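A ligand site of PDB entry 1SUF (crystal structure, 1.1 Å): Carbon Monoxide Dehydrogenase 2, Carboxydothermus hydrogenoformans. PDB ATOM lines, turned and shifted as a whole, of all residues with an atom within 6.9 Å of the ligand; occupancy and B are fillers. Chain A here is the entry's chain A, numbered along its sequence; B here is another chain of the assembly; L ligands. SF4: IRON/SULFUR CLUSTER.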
ATOM      1  N   CYS A  47      32.853  -4.540 -13.001  1.00  0.00           N
ATOM      2  CA  CYS A  47      31.465  -4.068 -13.128  1.00  0.00           C
ATOM      3  C   CYS A  47      30.580  -5.269 -12.822  1.00  0.00           C
ATOM      4  O   CYS A  47      30.914  -6.383 -13.274  1.00  0.00           O
ATOM      5  CB  CYS A  47      31.168  -3.527 -14.518  1.00  0.00           C
ATOM      6  SG  CYS A  47      29.410  -3.020 -14.701  1.00  0.00           S
ATOM      7  N   CYS A  48      29.482  -5.006 -12.110  1.00  0.00           N
ATOM      8  CA  CYS A  48      28.514  -6.043 -11.791  1.00  0.00           C
ATOM      9  C   CYS A  48      27.091  -5.509 -11.997  1.00  0.00           C
ATOM     10  O   CYS A  48      26.800  -4.428 -11.476  1.00  0.00           O
ATOM     11  CB  CYS A  48      28.714  -6.562 -10.367  1.00  0.00           C
ATOM     12  SG  CYS A  48      27.494  -7.841  -9.888  1.00  0.00           S
ATOM     13  N   ARG A  49      26.269  -6.302 -12.674  1.00  0.00           N
ATOM     14  CA  ARG A  49      24.841  -5.976 -12.890  1.00  0.00           C
ATOM     15  C   ARG A  49      23.979  -7.151 -12.455  1.00  0.00           C
ATOM     16  O   ARG A  49      22.913  -7.390 -12.984  1.00  0.00           O
ATOM     17  CB  ARG A  49      24.579  -5.638 -14.361  1.00  0.00           C
ATOM     18  CG  ARG A  49      25.264  -4.363 -14.770  1.00  0.00           C
ATOM     19  CD  ARG A  49      25.243  -4.155 -16.260  1.00  0.00           C
ATOM     20  NE  ARG A  49      23.926  -4.196 -16.780  1.00  0.00           N
ATOM     21  CZ  ARG A  49      23.470  -4.453 -17.983  1.00  0.00           C
ATOM     22  NH1 ARG A  49      24.293  -4.715 -18.985  1.00  0.00           N
ATOM     23  NH2 ARG A  49      22.140  -4.411 -18.142  1.00  0.00           N
ATOM     24  N   HIS A  50      24.478  -7.900 -11.462  1.00  0.00           N
ATOM     25  CA  HIS A  50      23.710  -9.106 -11.061  1.00  0.00           C
ATOM     26  C   HIS A  50      22.527  -8.834 -10.165  1.00  0.00           C
ATOM     27  O   HIS A  50      21.822  -9.809  -9.826  1.00  0.00           O
ATOM     28  CB  HIS A  50      24.634 -10.156 -10.415  1.00  0.00           C
ATOM     29  CG  HIS A  50      25.663 -10.694 -11.385  1.00  0.00           C
ATOM     30  ND1 HIS A  50      26.381 -11.850 -11.091  1.00  0.00           N
ATOM     31  CD2 HIS A  50      26.089 -10.281 -12.592  1.00  0.00           C
ATOM     32  CE1 HIS A  50      27.218 -12.105 -12.083  1.00  0.00           C
ATOM     33  NE2 HIS A  50      27.085 -11.180 -13.010  1.00  0.00           N
ATOM     34  N   CYS A  51      22.244  -7.590  -9.765  1.00  0.00           N
ATOM     35  CA  CYS A  51      20.928  -7.342  -9.144  1.00  0.00           C
ATOM     36  C   CYS A  51      20.492  -5.931  -9.450  1.00  0.00           C
ATOM     37  O   CYS A  51      21.256  -5.168 -10.030  1.00  0.00           O
ATOM     38  CB  CYS A  51      20.941  -7.577  -7.603  1.00  0.00           C
ATOM     39  SG  CYS A  51      21.727  -6.284  -6.615  1.00  0.00           S
ATOM     40  N   LEU A  52      19.275  -5.613  -9.033  1.00  0.00           N
ATOM     41  CA  LEU A  52      18.682  -4.298  -9.342  1.00  0.00           C
ATOM     42  C   LEU A  52      19.144  -3.184  -8.410  1.00  0.00           C
ATOM     43  O   LEU A  52      18.676  -2.055  -8.564  1.00  0.00           O
ATOM     44  CB  LEU A  52      17.145  -4.397  -9.322  1.00  0.00           C
ATOM     45  CG  LEU A  52      16.598  -5.369 -10.381  1.00  0.00           C
ATOM     46  CD1 LEU A  52      15.082  -5.524 -10.152  1.00  0.00           C
ATOM     47  CD2 LEU A  52      16.933  -4.982 -11.815  1.00  0.00           C
ATOM     48  N   GLN A  53      20.080  -3.487  -7.505  1.00  0.00           N
ATOM     49  CA  GLN A  53      20.764  -2.375  -6.813  1.00  0.00           C
ATOM     50  C   GLN A  53      21.894  -1.819  -7.637  1.00  0.00           C
ATOM     51  O   GLN A  53      22.380  -0.712  -7.407  1.00  0.00           O
ATOM     52  CB  GLN A  53      21.324  -2.791  -5.433  1.00  0.00           C
ATOM     53  CG  GLN A  53      20.178  -3.152  -4.497  1.00  0.00           C
ATOM     54  CD  GLN A  53      20.642  -3.631  -3.144  1.00  0.00           C
ATOM     55  OE1 GLN A  53      21.757  -4.234  -2.976  1.00  0.00           O
ATOM     56  NE2 GLN A  53      19.837  -3.408  -2.142  1.00  0.00           N
ATOM     57  N   GLY A  54      22.319  -2.592  -8.644  1.00  0.00           N
ATOM     58  CA  GLY A  54      23.370  -2.137  -9.525  1.00  0.00           C
ATOM     59  C   GLY A  54      22.881  -1.129 -10.559  1.00  0.00           C
ATOM     60  O   GLY A  54      21.721  -0.687 -10.534  1.00  0.00           O
ATOM     61  N   PRO A  55      23.738  -0.748 -11.503  1.00  0.00           N
ATOM     62  CA  PRO A  55      25.096  -1.299 -11.735  1.00  0.00           C
ATOM     63  C   PRO A  55      26.108  -0.837 -10.704  1.00  0.00           C
ATOM     64  O   PRO A  55      26.074   0.296 -10.233  1.00  0.00           O
ATOM     65  CB  PRO A  55      25.415  -0.771 -13.149  1.00  0.00           C
ATOM     66  CG  PRO A  55      24.706   0.575 -13.163  1.00  0.00           C
ATOM     67  CD  PRO A  55      23.382   0.279 -12.501  1.00  0.00           C
ATOM     68  N   CYS A  56      26.933  -1.805 -10.304  1.00  0.00           N
ATOM     69  CA  CYS A  56      28.079  -1.525  -9.428  1.00  0.00           C
ATOM     70  C   CYS A  56      29.362  -1.596 -10.218  1.00  0.00           C
ATOM     71  O   CYS A  56      29.494  -2.336 -11.183  1.00  0.00           O
ATOM     72  CB  CYS A  56      28.126  -2.545  -8.308  1.00  0.00           C
ATOM     73  SG  CYS A  56      26.777  -2.372  -7.075  1.00  0.00           S
ATOM     74  N   ARG A  57      30.334  -0.802  -9.766  1.00  0.00           N
ATOM     75  CA  ARG A  57      31.665  -0.782 -10.358  1.00  0.00           C
ATOM     76  C   ARG A  57      32.650  -0.572  -9.245  1.00  0.00           C
ATOM     77  O   ARG A  57      32.316  -0.111  -8.152  1.00  0.00           O
ATOM     78  CB  ARG A  57      31.752   0.290 -11.453  1.00  0.00           C
ATOM     79  CG  ARG A  57      31.769   1.692 -10.875  1.00  0.00           C
ATOM     80  CD  ARG A  57      31.334   2.798 -11.881  1.00  0.00           C
ATOM     81  NE  ARG A  57      31.577   4.106 -11.191  1.00  0.00           N
ATOM     82  CZ  ARG A  57      30.723   4.576 -10.278  1.00  0.00           C
ATOM     83  NH1 ARG A  57      30.986   5.729  -9.659  1.00  0.00           N
ATOM     84  NH2 ARG A  57      29.561   3.949  -9.972  1.00  0.00           N
ATOM     85  N   VAL A  67      34.144  -1.284  -3.468  1.00  0.00           N
ATOM     86  CA  VAL A  67      33.419  -2.537  -3.168  1.00  0.00           C
ATOM     87  C   VAL A  67      32.018  -2.414  -3.714  1.00  0.00           C
ATOM     88  O   VAL A  67      31.485  -1.295  -3.795  1.00  0.00           O
ATOM     89  CB  VAL A  67      33.508  -2.798  -1.650  1.00  0.00           C
ATOM     90  CG1 VAL A  67      32.864  -1.672  -0.846  1.00  0.00           C
ATOM     91  CG2 VAL A  67      32.839  -4.088  -1.242  1.00  0.00           C
ATOM     92  N   GLY A  68      31.389  -3.519  -4.109  1.00  0.00           N
ATOM     93  CA  GLY A  68      29.992  -3.459  -4.556  1.00  0.00           C
ATOM     94  C   GLY A  68      29.041  -3.154  -3.398  1.00  0.00           C
ATOM     95  O   GLY A  68      29.372  -3.277  -2.230  1.00  0.00           O
ATOM     96  N   ILE A  69      27.846  -2.770  -3.803  1.00  0.00           N
ATOM     97  CA  ILE A  69      26.872  -2.323  -2.785  1.00  0.00           C
ATOM     98  C   ILE A  69      26.554  -3.415  -1.791  1.00  0.00           C
ATOM     99  O   ILE A  69      26.446  -3.142  -0.606  1.00  0.00           O
ATOM    100  CB  ILE A  69      25.599  -1.791  -3.477  1.00  0.00           C
ATOM    101  CG1 ILE A  69      25.905  -0.449  -4.171  1.00  0.00           C
ATOM    102  CG2 ILE A  69      24.466  -1.639  -2.463  1.00  0.00           C
ATOM    103  CD1 ILE A  69      24.834   0.056  -5.111  1.00  0.00           C
ATOM    104  N   CYS A  70      26.479  -4.690  -2.227  1.00  0.00           N
ATOM    105  CA  CYS A  70      26.200  -5.785  -1.274  1.00  0.00           C
ATOM    106  C   CYS A  70      27.444  -6.222  -0.511  1.00  0.00           C
ATOM    107  O   CYS A  70      27.315  -7.136   0.336  1.00  0.00           O
ATOM    108  CB  CYS A  70      25.667  -7.000  -2.062  1.00  0.00           C
ATOM    109  SG  CYS A  70      26.907  -7.569  -3.321  1.00  0.00           S
ATOM    110  N   GLY A  71      28.604  -5.636  -0.777  1.00  0.00           N
ATOM    111  CA  GLY A  71      29.886  -6.035  -0.185  1.00  0.00           C
ATOM    112  C   GLY A  71      30.713  -6.907  -1.117  1.00  0.00           C
ATOM    113  O   GLY A  71      31.779  -7.365  -0.707  1.00  0.00           O
ATOM    114  N   ALA A  72      30.287  -7.164  -2.351  1.00  0.00           N
ATOM    115  CA  ALA A  72      31.096  -7.998  -3.272  1.00  0.00           C
ATOM    116  C   ALA A  72      32.412  -7.284  -3.573  1.00  0.00           C
ATOM    117  O   ALA A  72      32.445  -6.133  -4.007  1.00  0.00           O
ATOM    118  CB  ALA A  72      30.304  -8.241  -4.562  1.00  0.00           C
ATOM    119  N   THR A  73      33.510  -8.008  -3.355  1.00  0.00           N
ATOM    120  CA  THR A  73      34.822  -7.440  -3.626  1.00  0.00           C
ATOM    121  C   THR A  73      35.206  -7.511  -5.092  1.00  0.00           C
ATOM    122  O   THR A  73      34.546  -8.181  -5.896  1.00  0.00           O
ATOM    123  CB  THR A  73      35.878  -8.204  -2.806  1.00  0.00           C
ATOM    124  OG1 THR A  73      35.840  -9.555  -3.283  1.00  0.00           O
ATOM    125  CG2 THR A  73      35.641  -8.169  -1.305  1.00  0.00           C
ATOM    126  N   ILE A  77      33.597 -10.086  -7.839  1.00  0.00           N
ATOM    127  CA  ILE A  77      32.968  -9.614  -9.066  1.00  0.00           C
ATOM    128  C   ILE A  77      33.692 -10.151 -10.304  1.00  0.00           C
ATOM    129  O   ILE A  77      33.005 -10.666 -11.228  1.00  0.00           O
ATOM    130  CB  ILE A  77      32.892  -8.074  -9.055  1.00  0.00           C
ATOM    131  CG1 ILE A  77      31.846  -7.593  -8.025  1.00  0.00           C
ATOM    132  CG2 ILE A  77      32.617  -7.499 -10.436  1.00  0.00           C
ATOM    133  CD1 ILE A  77      31.880  -6.056  -7.888  1.00  0.00           C
ATOM    134  N   ARG A  80      32.931 -13.958 -10.660  1.00  0.00           N
ATOM    135  CA  ARG A  80      31.539 -14.245 -11.017  1.00  0.00           C
ATOM    136  C   ARG A  80      31.309 -13.938 -12.489  1.00  0.00           C
ATOM    137  O   ARG A  80      30.652 -14.743 -13.173  1.00  0.00           O
ATOM    138  CB  ARG A  80      30.560 -13.409 -10.169  1.00  0.00           C
ATOM    139  CG  ARG A  80      30.576 -13.825  -8.678  1.00  0.00           C
ATOM    140  CD  ARG A  80      29.350 -13.288  -7.891  1.00  0.00           C
ATOM    141  NE  ARG A  80      29.270 -11.812  -8.000  1.00  0.00           N
ATOM    142  CZ  ARG A  80      28.544 -11.101  -7.172  1.00  0.00           C
ATOM    143  NH1 ARG A  80      27.859 -11.706  -6.154  1.00  0.00           N
ATOM    144  NH2 ARG A  80      28.446  -9.777  -7.270  1.00  0.00           N
ATOM    145  N   THR A 197      26.673 -17.572  -8.833  1.00  0.00           N
ATOM    146  CA  THR A 197      27.153 -16.251  -9.214  1.00  0.00           C
ATOM    147  C   THR A 197      26.061 -15.167  -9.043  1.00  0.00           C
ATOM    148  O   THR A 197      26.356 -13.982  -9.226  1.00  0.00           O
ATOM    149  CB  THR A 197      27.701 -16.176 -10.656  1.00  0.00           C
ATOM    150  OG1 THR A 197      26.650 -16.614 -11.555  1.00  0.00           O
ATOM    151  CG2 THR A 197      28.928 -17.073 -10.832  1.00  0.00           C
ATOM    152  N   SER A 198      24.848 -15.598  -8.715  1.00  0.00           N
ATOM    153  CA  SER A 198      23.766 -14.653  -8.464  1.00  0.00           C
ATOM    154  C   SER A 198      24.007 -13.945  -7.113  1.00  0.00           C
ATOM    155  O   SER A 198      24.870 -14.362  -6.316  1.00  0.00           O
ATOM    156  CB  SER A 198      22.413 -15.338  -8.551  1.00  0.00           C
ATOM    157  OG  SER A 198      22.107 -16.149  -7.438  1.00  0.00           O
ATOM    158  N   MET A 199      23.235 -12.890  -6.845  1.00  0.00           N
ATOM    159  CA  MET A 199      23.557 -12.074  -5.677  1.00  0.00           C
ATOM    160  C   MET A 199      23.438 -12.880  -4.391  1.00  0.00           C
ATOM    161  O   MET A 199      22.495 -13.664  -4.173  1.00  0.00           O
ATOM    162  CB  MET A 199      22.606 -10.828  -5.682  1.00  0.00           C
ATOM    163  CG  MET A 199      22.880  -9.902  -4.493  1.00  0.00           C
ATOM    164  SD  MET A 199      21.953 -10.399  -3.016  1.00  0.00           S
ATOM    165  CE  MET A 199      22.981  -9.759  -1.685  1.00  0.00           C
ATOM    166  N   GLY A 200      24.407 -12.626  -3.498  1.00  0.00           N
ATOM    167  CA  GLY A 200      24.295 -13.192  -2.162  1.00  0.00           C
ATOM    168  C   GLY A 200      24.572 -14.679  -2.031  1.00  0.00           C
ATOM    169  O   GLY A 200      24.117 -15.285  -1.051  1.00  0.00           O
ATOM    170  N   VAL B  28      25.493  -1.275   3.952  1.00  0.00           N
ATOM    171  CA  VAL B  28      25.002  -1.260   2.560  1.00  0.00           C
ATOM    172  C   VAL B  28      24.597   0.128   2.123  1.00  0.00           C
ATOM    173  O   VAL B  28      24.857   0.480   0.962  1.00  0.00           O
ATOM    174  CB  VAL B  28      23.819  -2.264   2.476  1.00  0.00           C
ATOM    175  CG1 VAL B  28      22.602  -1.835   3.323  1.00  0.00           C
ATOM    176  CG2 VAL B  28      23.428  -2.483   1.011  1.00  0.00           C
ATOM    177  N   MET B  35      28.773   4.557  -4.378  1.00  0.00           N
ATOM    178  CA  MET B  35      28.644   4.127  -5.754  1.00  0.00           C
ATOM    179  C   MET B  35      28.046   5.204  -6.633  1.00  0.00           C
ATOM    180  O   MET B  35      28.050   5.070  -7.854  1.00  0.00           O
ATOM    181  CB  MET B  35      27.746   2.863  -5.768  1.00  0.00           C
ATOM    182  CG  MET B  35      27.872   2.078  -7.063  1.00  0.00           C
ATOM    183  SD  MET B  35      29.545   1.434  -7.367  1.00  0.00           S
ATOM    184  CE  MET B  35      29.650   0.219  -6.068  1.00  0.00           C
ATOM    185  N   GLN B  38      25.583   6.219 -10.352  1.00  0.00           N
ATOM    186  CA  GLN B  38      25.719   4.904 -10.976  1.00  0.00           C
ATOM    187  C   GLN B  38      25.741   5.054 -12.508  1.00  0.00           C
ATOM    188  O   GLN B  38      25.260   6.034 -13.091  1.00  0.00           O
ATOM    189  CB  GLN B  38      24.582   3.976 -10.491  1.00  0.00           C
ATOM    190  CG  GLN B  38      24.789   3.571  -9.037  1.00  0.00           C
ATOM    191  CD  GLN B  38      23.756   2.601  -8.505  1.00  0.00           C
ATOM    192  OE1 GLN B  38      23.977   1.372  -8.472  1.00  0.00           O
ATOM    193  NE2 GLN B  38      22.612   3.116  -8.122  1.00  0.00           N
ATOM    194  N   PRO B 336      27.663 -10.330   1.207  1.00  0.00           N
ATOM    195  CA  PRO B 336      28.960 -10.894   1.668  1.00  0.00           C
ATOM    196  C   PRO B 336      29.662  -9.952   2.631  1.00  0.00           C
ATOM    197  O   PRO B 336      30.600 -10.385   3.315  1.00  0.00           O
ATOM    198  CB  PRO B 336      29.721 -11.118   0.368  1.00  0.00           C
ATOM    199  CG  PRO B 336      29.123 -10.158  -0.621  1.00  0.00           C
ATOM    200  CD  PRO B 336      27.633 -10.152  -0.293  1.00  0.00           C
ATOM    201  N   MET B 560      14.904  -6.564  -5.940  1.00  0.00           N
ATOM    202  CA  MET B 560      16.385  -6.533  -6.018  1.00  0.00           C
ATOM    203  C   MET B 560      16.944  -7.725  -6.808  1.00  0.00           C
ATOM    204  O   MET B 560      17.719  -7.560  -7.769  1.00  0.00           O
ATOM    205  CB  MET B 560      16.981  -6.455  -4.590  1.00  0.00           C
ATOM    206  CG  MET B 560      18.492  -6.473  -4.538  1.00  0.00           C
ATOM    207  SD  MET B 560      19.260  -8.110  -4.355  1.00  0.00           S
ATOM    208  CE  MET B 560      18.501  -8.682  -2.804  1.00  0.00           C
HETATM  209 FE1  SF4 L   1      26.240  -6.823  -5.387  1.00  0.00          FE
HETATM  210 FE2  SF4 L   1      26.366  -6.923  -8.124  1.00  0.00          FE
HETATM  211 FE3  SF4 L   1      26.015  -4.562  -6.923  1.00  0.00          FE
HETATM  212 FE4  SF4 L   1      23.977  -6.317  -6.962  1.00  0.00          FE
HETATM  213  S1  SF4 L   1      24.844  -5.321  -8.758  1.00  0.00           S
HETATM  214  S2  SF4 L   1      24.710  -5.059  -5.150  1.00  0.00           S
HETATM  215  S3  SF4 L   1      25.170  -8.324  -6.815  1.00  0.00           S
HETATM  216  S4  SF4 L   1      27.853  -5.957  -6.682  1.00  0.00           S
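The backbone NH (N) of Cys 51 sits close to a sulfur (S1) of the ligand, at 3.6 Å. FE4 of the ligand is bound by SG of Cys 51 (2.3 Å). SG of Cys 48 binds FE2 of the ligand. S2 of the ligand sits close to N of Cys 70 (3.4 Å). The side-chain sulfur of Cys 70 is bound to an iron atom (FE1) of the ligand. The side-chain sulfur (SG) of Cys 56 binds an iron atom (FE3) of the ligand, 2.3 Å away. The backbone NH (N) of Gly 54 sits close to a sulfur (S1) of the ligand (3.7 Å). S3 of the ligand sits close to NH2 of Arg 80, at 3.6 Å. A sulfur (S1) of the ligand sits close to the backbone NH (N) of His 50. The side-chain amide oxygen (OE1) of Gln 53 lies close to a sulfur (S2) of the ligand (3.8 Å).
The backbone NH (N) of Gln 53 sits close to the side-chain sulfur (SG) of Cys 51 (3.4 Å). The backbone NH (N) of Cys 48 sits at hydrogen-bond distance from the backbone carbonyl oxygen (O) of Cys 56 (2.8 Å). SG of Cys 48 lies close to NH2 of Arg 80. The backbone NH (N) of His 50 sits close to the side-chain sulfur (SG) of Cys 48 (3.4 Å). The side-chain sulfur (SG) of Cys 70 sits close to the backbone NH (N) of Ala 72, at 3.5 Å. The side-chain sulfur of Cys 56 sits close to the backbone NH of Ile 69 (3.5 Å). O of Thr 197 sits at hydrogen-bond distance from ND1 of His 50 (2.8 Å). O of Gln 53 lies close to OE1 of Gln 38 of chain B (2.8 Å).
Gly 68 touches the ligand (CA to S4, 3.9 Å). Ile 69 touches the ligand. Ala 72 touches the ligand. Met 199 touches the ligand. Hydrophobic or aromatic side chains within 4 Å of the ligand: Ile 69, Ala 72 and Met 199. The nearest printed residue that does not touch the ligand is Arg 49 (4.2 Å).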
